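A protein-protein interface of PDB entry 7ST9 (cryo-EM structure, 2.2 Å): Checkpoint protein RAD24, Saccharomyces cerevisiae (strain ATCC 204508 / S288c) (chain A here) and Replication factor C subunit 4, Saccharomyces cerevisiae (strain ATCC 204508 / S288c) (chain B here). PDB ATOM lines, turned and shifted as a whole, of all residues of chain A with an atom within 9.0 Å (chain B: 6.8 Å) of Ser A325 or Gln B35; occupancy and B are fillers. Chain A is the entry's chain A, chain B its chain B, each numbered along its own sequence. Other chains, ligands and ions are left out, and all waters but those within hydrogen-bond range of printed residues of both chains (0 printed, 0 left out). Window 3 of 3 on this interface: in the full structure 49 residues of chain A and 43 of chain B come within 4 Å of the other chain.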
ATOM      1  N   MET A 287      31.028 -13.182 -12.770  1.00  0.00           N
ATOM      2  CA  MET A 287      30.059 -12.104 -12.945  1.00  0.00           C
ATOM      3  C   MET A 287      28.981 -12.485 -13.953  1.00  0.00           C
ATOM      4  O   MET A 287      27.804 -12.159 -13.761  1.00  0.00           O
ATOM      5  CB  MET A 287      30.776 -10.819 -13.363  1.00  0.00           C
ATOM      6  CG  MET A 287      31.571 -10.911 -14.660  1.00  0.00           C
ATOM      7  SD  MET A 287      31.376  -9.455 -15.704  1.00  0.00           S
ATOM      8  CE  MET A 287      29.670  -9.627 -16.221  1.00  0.00           C
ATOM      9  N   LYS A 291      25.012 -12.594 -13.090  1.00  0.00           N
ATOM     10  CA  LYS A 291      24.045 -11.791 -13.826  1.00  0.00           C
ATOM     11  C   LYS A 291      23.135 -12.624 -14.721  1.00  0.00           C
ATOM     12  O   LYS A 291      22.234 -12.061 -15.352  1.00  0.00           O
ATOM     13  CB  LYS A 291      24.777 -10.742 -14.667  1.00  0.00           C
ATOM     14  CG  LYS A 291      23.938  -9.509 -14.986  1.00  0.00           C
ATOM     15  CD  LYS A 291      24.680  -8.495 -15.856  1.00  0.00           C
ATOM     16  CE  LYS A 291      26.078  -8.185 -15.334  1.00  0.00           C
ATOM     17  NZ  LYS A 291      26.064  -7.770 -13.904  1.00  0.00           N
ATOM     18  N   ASN A 292      23.347 -13.935 -14.797  1.00  0.00           N
ATOM     19  CA  ASN A 292      22.523 -14.898 -15.525  1.00  0.00           C
ATOM     20  C   ASN A 292      22.756 -14.849 -17.031  1.00  0.00           C
ATOM     21  O   ASN A 292      22.181 -15.676 -17.751  1.00  0.00           O
ATOM     22  CB  ASN A 292      21.022 -14.701 -15.257  1.00  0.00           C
ATOM     23  CG  ASN A 292      20.195 -15.906 -15.659  1.00  0.00           C
ATOM     24  OD1 ASN A 292      19.530 -15.900 -16.695  1.00  0.00           O
ATOM     25  ND2 ASN A 292      20.233 -16.951 -14.839  1.00  0.00           N
ATOM     26  N   LYS A 293      23.572 -13.924 -17.538  1.00  0.00           N
ATOM     27  CA  LYS A 293      23.838 -13.854 -18.969  1.00  0.00           C
ATOM     28  C   LYS A 293      24.777 -14.952 -19.452  1.00  0.00           C
ATOM     29  O   LYS A 293      24.903 -15.148 -20.666  1.00  0.00           O
ATOM     30  CB  LYS A 293      24.429 -12.487 -19.325  1.00  0.00           C
ATOM     31  CG  LYS A 293      23.386 -11.431 -19.652  1.00  0.00           C
ATOM     32  CD  LYS A 293      24.030 -10.098 -20.001  1.00  0.00           C
ATOM     33  CE  LYS A 293      22.989  -9.075 -20.425  1.00  0.00           C
ATOM     34  NZ  LYS A 293      23.601  -7.767 -20.789  1.00  0.00           N
ATOM     35  N   GLN A 319      32.043  -6.447 -23.694  1.00  0.00           N
ATOM     36  CA  GLN A 319      32.025  -5.817 -22.377  1.00  0.00           C
ATOM     37  C   GLN A 319      30.748  -5.013 -22.176  1.00  0.00           C
ATOM     38  O   GLN A 319      30.122  -5.082 -21.111  1.00  0.00           O
ATOM     39  CB  GLN A 319      33.252  -4.922 -22.205  1.00  0.00           C
ATOM     40  CG  GLN A 319      33.354  -4.272 -20.834  1.00  0.00           C
ATOM     41  CD  GLN A 319      34.657  -3.523 -20.637  1.00  0.00           C
ATOM     42  OE1 GLN A 319      35.376  -3.244 -21.597  1.00  0.00           O
ATOM     43  NE2 GLN A 319      34.968  -3.194 -19.390  1.00  0.00           N
ATOM     44  N   PHE A 320      30.345  -4.245 -23.190  1.00  0.00           N
ATOM     45  CA  PHE A 320      29.136  -3.440 -23.069  1.00  0.00           C
ATOM     46  C   PHE A 320      27.909  -4.321 -22.867  1.00  0.00           C
ATOM     47  O   PHE A 320      27.041  -4.011 -22.045  1.00  0.00           O
ATOM     48  CB  PHE A 320      28.969  -2.558 -24.307  1.00  0.00           C
ATOM     49  CG  PHE A 320      28.025  -1.406 -24.110  1.00  0.00           C
ATOM     50  CD1 PHE A 320      28.248  -0.469 -23.114  1.00  0.00           C
ATOM     51  CD2 PHE A 320      26.915  -1.258 -24.923  1.00  0.00           C
ATOM     52  CE1 PHE A 320      27.383   0.590 -22.934  1.00  0.00           C
ATOM     53  CE2 PHE A 320      26.045  -0.200 -24.747  1.00  0.00           C
ATOM     54  CZ  PHE A 320      26.279   0.726 -23.751  1.00  0.00           C
ATOM     55  N   TRP A 321      27.819  -5.425 -23.613  1.00  0.00           N
ATOM     56  CA  TRP A 321      26.686  -6.330 -23.450  1.00  0.00           C
ATOM     57  C   TRP A 321      26.685  -6.976 -22.070  1.00  0.00           C
ATOM     58  O   TRP A 321      25.633  -7.076 -21.428  1.00  0.00           O
ATOM     59  CB  TRP A 321      26.711  -7.402 -24.539  1.00  0.00           C
ATOM     60  CG  TRP A 321      25.972  -8.650 -24.159  1.00  0.00           C
ATOM     61  CD1 TRP A 321      24.630  -8.871 -24.259  1.00  0.00           C
ATOM     62  CD2 TRP A 321      26.537  -9.848 -23.614  1.00  0.00           C
ATOM     63  NE1 TRP A 321      24.324 -10.133 -23.812  1.00  0.00           N
ATOM     64  CE2 TRP A 321      25.477 -10.753 -23.410  1.00  0.00           C
ATOM     65  CE3 TRP A 321      27.834 -10.244 -23.278  1.00  0.00           C
ATOM     66  CZ2 TRP A 321      25.675 -12.029 -22.887  1.00  0.00           C
ATOM     67  CZ3 TRP A 321      28.030 -11.510 -22.760  1.00  0.00           C
ATOM     68  CH2 TRP A 321      26.955 -12.388 -22.569  1.00  0.00           C
ATOM     69  N   ALA A 322      27.850  -7.421 -21.597  1.00  0.00           N
ATOM     70  CA  ALA A 322      27.907  -8.133 -20.325  1.00  0.00           C
ATOM     71  C   ALA A 322      27.584  -7.207 -19.158  1.00  0.00           C
ATOM     72  O   ALA A 322      26.794  -7.558 -18.275  1.00  0.00           O
ATOM     73  CB  ALA A 322      29.285  -8.767 -20.141  1.00  0.00           C
ATOM     74  N   THR A 323      28.186  -6.015 -19.139  1.00  0.00           N
ATOM     75  CA  THR A 323      27.972  -5.095 -18.029  1.00  0.00           C
ATOM     76  C   THR A 323      26.530  -4.609 -17.948  1.00  0.00           C
ATOM     77  O   THR A 323      26.102  -4.154 -16.882  1.00  0.00           O
ATOM     78  CB  THR A 323      28.915  -3.897 -18.150  1.00  0.00           C
ATOM     79  OG1 THR A 323      30.260  -4.360 -18.324  1.00  0.00           O
ATOM     80  CG2 THR A 323      28.842  -3.025 -16.904  1.00  0.00           C
ATOM     81  N   SER A 324      25.773  -4.697 -19.039  1.00  0.00           N
ATOM     82  CA  SER A 324      24.397  -4.218 -19.055  1.00  0.00           C
ATOM     83  C   SER A 324      23.474  -5.280 -18.469  1.00  0.00           C
ATOM     84  O   SER A 324      23.438  -6.416 -18.954  1.00  0.00           O
ATOM     85  CB  SER A 324      23.973  -3.870 -20.480  1.00  0.00           C
ATOM     86  OG  SER A 324      23.523  -5.020 -21.172  1.00  0.00           O
ATOM     87  N   SER A 325      22.729  -4.911 -17.424  1.00  0.00           N
ATOM     88  CA  SER A 325      21.761  -5.839 -16.851  1.00  0.00           C
ATOM     89  C   SER A 325      20.544  -6.002 -17.753  1.00  0.00           C
ATOM     90  O   SER A 325      19.916  -7.067 -17.757  1.00  0.00           O
ATOM     91  CB  SER A 325      21.333  -5.362 -15.462  1.00  0.00           C
ATOM     92  OG  SER A 325      20.576  -4.168 -15.541  1.00  0.00           O
ATOM     93  N   GLY A 326      20.201  -4.969 -18.520  1.00  0.00           N
ATOM     94  CA  GLY A 326      19.097  -5.030 -19.452  1.00  0.00           C
ATOM     95  C   GLY A 326      19.511  -5.615 -20.789  1.00  0.00           C
ATOM     96  O   GLY A 326      20.600  -6.168 -20.956  1.00  0.00           O
ATOM     97  N   SER A 327      18.612  -5.484 -21.761  1.00  0.00           N
ATOM     98  CA  SER A 327      18.820  -5.996 -23.109  1.00  0.00           C
ATOM     99  C   SER A 327      18.853  -4.835 -24.091  1.00  0.00           C
ATOM    100  O   SER A 327      17.966  -3.974 -24.072  1.00  0.00           O
ATOM    101  CB  SER A 327      17.718  -6.986 -23.496  1.00  0.00           C
ATOM    102  OG  SER A 327      16.474  -6.329 -23.656  1.00  0.00           O
ATOM    103  N   LEU A 328      19.868  -4.816 -24.943  1.00  0.00           N
ATOM    104  CA  LEU A 328      20.048  -3.805 -25.970  1.00  0.00           C
ATOM    105  C   LEU A 328      20.432  -4.477 -27.278  1.00  0.00           C
ATOM    106  O   LEU A 328      20.953  -5.597 -27.280  1.00  0.00           O
ATOM    107  CB  LEU A 328      21.135  -2.793 -25.579  1.00  0.00           C
ATOM    108  CG  LEU A 328      20.721  -1.581 -24.743  1.00  0.00           C
ATOM    109  CD1 LEU A 328      21.954  -0.783 -24.362  1.00  0.00           C
ATOM    110  CD2 LEU A 328      19.727  -0.700 -25.484  1.00  0.00           C
ATOM    111  N   LEU B  20      18.296  12.408 -16.405  1.00  0.00           N
ATOM    112  CA  LEU B  20      17.989  11.356 -17.366  1.00  0.00           C
ATOM    113  C   LEU B  20      16.558  10.859 -17.214  1.00  0.00           C
ATOM    114  O   LEU B  20      15.949  10.413 -18.195  1.00  0.00           O
ATOM    115  CB  LEU B  20      18.972  10.196 -17.198  1.00  0.00           C
ATOM    116  CG  LEU B  20      20.401  10.458 -17.683  1.00  0.00           C
ATOM    117  CD1 LEU B  20      21.352   9.401 -17.145  1.00  0.00           C
ATOM    118  CD2 LEU B  20      20.457  10.509 -19.201  1.00  0.00           C
ATOM    119  N   ILE B  30      18.062   4.815 -22.698  1.00  0.00           N
ATOM    120  CA  ILE B  30      18.099   5.702 -21.539  1.00  0.00           C
ATOM    121  C   ILE B  30      18.327   4.901 -20.263  1.00  0.00           C
ATOM    122  O   ILE B  30      19.012   5.358 -19.343  1.00  0.00           O
ATOM    123  CB  ILE B  30      16.809   6.539 -21.458  1.00  0.00           C
ATOM    124  CG1 ILE B  30      16.550   7.271 -22.781  1.00  0.00           C
ATOM    125  CG2 ILE B  30      16.898   7.537 -20.311  1.00  0.00           C
ATOM    126  CD1 ILE B  30      17.689   8.160 -23.240  1.00  0.00           C
ATOM    127  N   ASP B  31      17.750   3.699 -20.180  1.00  0.00           N
ATOM    128  CA  ASP B  31      17.987   2.849 -19.019  1.00  0.00           C
ATOM    129  C   ASP B  31      19.451   2.439 -18.931  1.00  0.00           C
ATOM    130  O   ASP B  31      20.034   2.419 -17.841  1.00  0.00           O
ATOM    131  CB  ASP B  31      17.087   1.615 -19.078  1.00  0.00           C
ATOM    132  CG  ASP B  31      16.669   1.128 -17.703  1.00  0.00           C
ATOM    133  OD1 ASP B  31      17.119   1.712 -16.694  1.00  0.00           O
ATOM    134  OD2 ASP B  31      15.887   0.156 -17.629  1.00  0.00           O
ATOM    135  N   ARG B  32      20.063   2.106 -20.069  1.00  0.00           N
ATOM    136  CA  ARG B  32      21.486   1.789 -20.070  1.00  0.00           C
ATOM    137  C   ARG B  32      22.313   2.995 -19.640  1.00  0.00           C
ATOM    138  O   ARG B  32      23.290   2.857 -18.893  1.00  0.00           O
ATOM    139  CB  ARG B  32      21.912   1.310 -21.459  1.00  0.00           C
ATOM    140  CG  ARG B  32      23.361   0.855 -21.554  1.00  0.00           C
ATOM    141  CD  ARG B  32      23.531  -0.569 -21.057  1.00  0.00           C
ATOM    142  NE  ARG B  32      24.935  -0.923 -20.885  1.00  0.00           N
ATOM    143  CZ  ARG B  32      25.638  -0.698 -19.783  1.00  0.00           C
ATOM    144  NH1 ARG B  32      25.100  -0.115 -18.723  1.00  0.00           N
ATOM    145  NH2 ARG B  32      26.915  -1.069 -19.741  1.00  0.00           N
ATOM    146  N   LEU B  33      21.939   4.189 -20.107  1.00  0.00           N
ATOM    147  CA  LEU B  33      22.656   5.392 -19.700  1.00  0.00           C
ATOM    148  C   LEU B  33      22.528   5.628 -18.199  1.00  0.00           C
ATOM    149  O   LEU B  33      23.500   6.005 -17.539  1.00  0.00           O
ATOM    150  CB  LEU B  33      22.140   6.602 -20.480  1.00  0.00           C
ATOM    151  CG  LEU B  33      22.535   6.679 -21.958  1.00  0.00           C
ATOM    152  CD1 LEU B  33      22.067   7.991 -22.562  1.00  0.00           C
ATOM    153  CD2 LEU B  33      24.039   6.511 -22.144  1.00  0.00           C
ATOM    154  N   GLN B  34      21.333   5.413 -17.644  1.00  0.00           N
ATOM    155  CA  GLN B  34      21.151   5.550 -16.202  1.00  0.00           C
ATOM    156  C   GLN B  34      21.985   4.525 -15.445  1.00  0.00           C
ATOM    157  O   GLN B  34      22.564   4.832 -14.395  1.00  0.00           O
ATOM    158  CB  GLN B  34      19.672   5.402 -15.844  1.00  0.00           C
ATOM    159  CG  GLN B  34      18.806   6.567 -16.293  1.00  0.00           C
ATOM    160  CD  GLN B  34      18.194   7.319 -15.129  1.00  0.00           C
ATOM    161  OE1 GLN B  34      18.870   8.090 -14.448  1.00  0.00           O
ATOM    162  NE2 GLN B  34      16.906   7.097 -14.892  1.00  0.00           N
ATOM    163  N   GLN B  35      22.045   3.294 -15.956  1.00  0.00           N
ATOM    164  CA  GLN B  35      22.883   2.269 -15.343  1.00  0.00           C
ATOM    165  C   GLN B  35      24.340   2.709 -15.317  1.00  0.00           C
ATOM    166  O   GLN B  35      25.022   2.593 -14.290  1.00  0.00           O
ATOM    167  CB  GLN B  35      22.739   0.954 -16.110  1.00  0.00           C
ATOM    168  CG  GLN B  35      21.632   0.046 -15.608  1.00  0.00           C
ATOM    169  CD  GLN B  35      21.906  -1.415 -15.903  1.00  0.00           C
ATOM    170  OE1 GLN B  35      21.024  -2.147 -16.352  1.00  0.00           O
ATOM    171  NE2 GLN B  35      23.133  -1.850 -15.641  1.00  0.00           N
ATOM    172  N   ILE B  36      24.835   3.222 -16.445  1.00  0.00           N
ATOM    173  CA  ILE B  36      26.213   3.700 -16.503  1.00  0.00           C
ATOM    174  C   ILE B  36      26.418   4.840 -15.515  1.00  0.00           C
ATOM    175  O   ILE B  36      27.427   4.893 -14.802  1.00  0.00           O
ATOM    176  CB  ILE B  36      26.569   4.127 -17.940  1.00  0.00           C
ATOM    177  CG1 ILE B  36      26.697   2.900 -18.843  1.00  0.00           C
ATOM    178  CG2 ILE B  36      27.860   4.931 -17.952  1.00  0.00           C
ATOM    179  CD1 ILE B  36      26.547   3.211 -20.316  1.00  0.00           C
ATOM    180  N   ALA B  37      25.461   5.767 -15.457  1.00  0.00           N
ATOM    181  CA  ALA B  37      25.592   6.918 -14.574  1.00  0.00           C
ATOM    182  C   ALA B  37      25.681   6.488 -13.116  1.00  0.00           C
ATOM    183  O   ALA B  37      26.491   7.025 -12.352  1.00  0.00           O
ATOM    184  CB  ALA B  37      24.411   7.865 -14.782  1.00  0.00           C
ATOM    185  N   LYS B  38      24.856   5.524 -12.711  1.00  0.00           N
ATOM    186  CA  LYS B  38      24.878   5.052 -11.333  1.00  0.00           C
ATOM    187  C   LYS B  38      26.015   4.076 -11.054  1.00  0.00           C
ATOM    188  O   LYS B  38      26.305   3.811  -9.883  1.00  0.00           O
ATOM    189  CB  LYS B  38      23.537   4.402 -10.975  1.00  0.00           C
ATOM    190  CG  LYS B  38      23.278   3.063 -11.645  1.00  0.00           C
ATOM    191  CD  LYS B  38      21.981   2.444 -11.145  1.00  0.00           C
ATOM    192  CE  LYS B  38      21.822   1.015 -11.634  1.00  0.00           C
ATOM    193  NZ  LYS B  38      20.638   0.346 -11.027  1.00  0.00           N
ATOM    194  N   ASP B  39      26.662   3.538 -12.090  1.00  0.00           N
ATOM    195  CA  ASP B  39      27.799   2.641 -11.899  1.00  0.00           C
ATOM    196  C   ASP B  39      29.118   3.412 -11.886  1.00  0.00           C
ATOM    197  O   ASP B  39      29.864   3.361 -10.904  1.00  0.00           O
ATOM    198  CB  ASP B  39      27.812   1.570 -12.994  1.00  0.00           C
ATOM    199  CG  ASP B  39      26.755   0.503 -12.781  1.00  0.00           C
ATOM    200  OD1 ASP B  39      26.028   0.579 -11.768  1.00  0.00           O
ATOM    201  OD2 ASP B  39      26.652  -0.410 -13.626  1.00  0.00           O
ATOM    202  N   GLY B  40      29.415   4.126 -12.971  1.00  0.00           N
ATOM    203  CA  GLY B  40      30.597   4.965 -13.024  1.00  0.00           C
ATOM    204  C   GLY B  40      31.562   4.619 -14.140  1.00  0.00           C
ATOM    205  O   GLY B  40      32.157   5.515 -14.747  1.00  0.00           O
ATOM    206  N   ASN B  41      31.725   3.329 -14.430  1.00  0.00           N
ATOM    207  CA  ASN B  41      32.708   2.896 -15.417  1.00  0.00           C
ATOM    208  C   ASN B  41      32.227   3.217 -16.826  1.00  0.00           C
ATOM    209  O   ASN B  41      31.849   2.318 -17.584  1.00  0.00           O
ATOM    210  CB  ASN B  41      32.986   1.397 -15.269  1.00  0.00           C
ATOM    211  CG  ASN B  41      33.968   0.868 -16.308  1.00  0.00           C
ATOM    212  OD1 ASN B  41      34.771   1.627 -16.850  1.00  0.00           O
ATOM    213  ND2 ASN B  41      33.899  -0.428 -16.601  1.00  0.00           N
ATOM    214  N   LEU B  62      24.086  12.772 -18.416  1.00  0.00           N
ATOM    215  CA  LEU B  62      24.948  11.697 -17.941  1.00  0.00           C
ATOM    216  C   LEU B  62      26.224  12.259 -17.330  1.00  0.00           C
ATOM    217  O   LEU B  62      26.647  11.835 -16.248  1.00  0.00           O
ATOM    218  CB  LEU B  62      25.271  10.743 -19.092  1.00  0.00           C
ATOM    219  CG  LEU B  62      26.387   9.724 -18.849  1.00  0.00           C
ATOM    220  CD1 LEU B  62      26.043   8.813 -17.684  1.00  0.00           C
ATOM    221  CD2 LEU B  62      26.644   8.911 -20.106  1.00  0.00           C
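The backbone NH (N) of Ser A325 sits close to the side-chain amide oxygen (OE1) of Gln B35, 3.4 Å away.
The side-chain hydroxyl (OG) of Ser A324 lies within hydrogen-bond range of the side-chain amino group (NZ) of Lys A293, 2.8 Å away. The backbone carbonyl oxygen (O) of Gly A326 sits at hydrogen-bond distance from the side-chain amino group (NZ) of Lys A293. O of Gln A319 lies within hydrogen-bond range of OG1 of Thr A323, 2.9 Å away. The side-chain hydroxyl of Ser A324 lies within hydrogen-bond range of the backbone carbonyl oxygen of Trp A321. O of Gly A326 sits at hydrogen-bond distance from OG of Ser A324 (3.1 Å).
Among the printed residues, pairs that only touch across the chains: Phe A320 with Arg B32, Phe A320 with Ile B36, Thr A323 with Arg B32, Thr A323 with Gln B35, Ser A324 with Arg B32, Gly A326 with Gln B35 and Leu A328 with Arg B32.
Printed residues of chain B within 4 Å of Phe A320: Arg B32 (3.5 Å) and Ile B36 (3.8 Å). Of the printed residues of chain B, Ser A324 touches Arg B32. Ser A325 touches one residue of chain B. Of the printed residues of chain B, Gly A326 touches Gln B35 (3.7 Å). Printed residues of chain A within 4 Å of Arg B32: Phe A320 (3.5 Å), Thr A323 (3.8 Å), Ser A324 (3.1 Å) and Leu A328 (3.5 Å). Leu B33 touches none of the printed residues of chain A. Gln B34 touches none of the printed residues of chain A. Gln B35 touches just these residues of chain A: Thr A323 (3.96 Å), Ser A325 (2.2 Å) and Gly A326 (3.7 Å). No residue of chain A comes within 4 Å of Lys B38. The nearest residue of chain A that does not touch Gln B35 is Ser A324 (4.3 Å).
Printed residues of chain A that touch a printed residue of chain B: Phe A320, Thr A323, Ser A324, Ser A325, Gly A326 and Leu A328. Hydrophobic or aromatic side chains of chain A within 4 Å of the printed part of chain B: Phe A320 and Leu A328. Of the 14 printed residues of chain B, 3 touch a printed residue of chain A. Among the printed residues, 8 pairs touch across the chains. Among the printed residues, no Asp or Glu carboxylate lies within 4 Å of a Lys or Arg side-chain nitrogen of the other chain.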
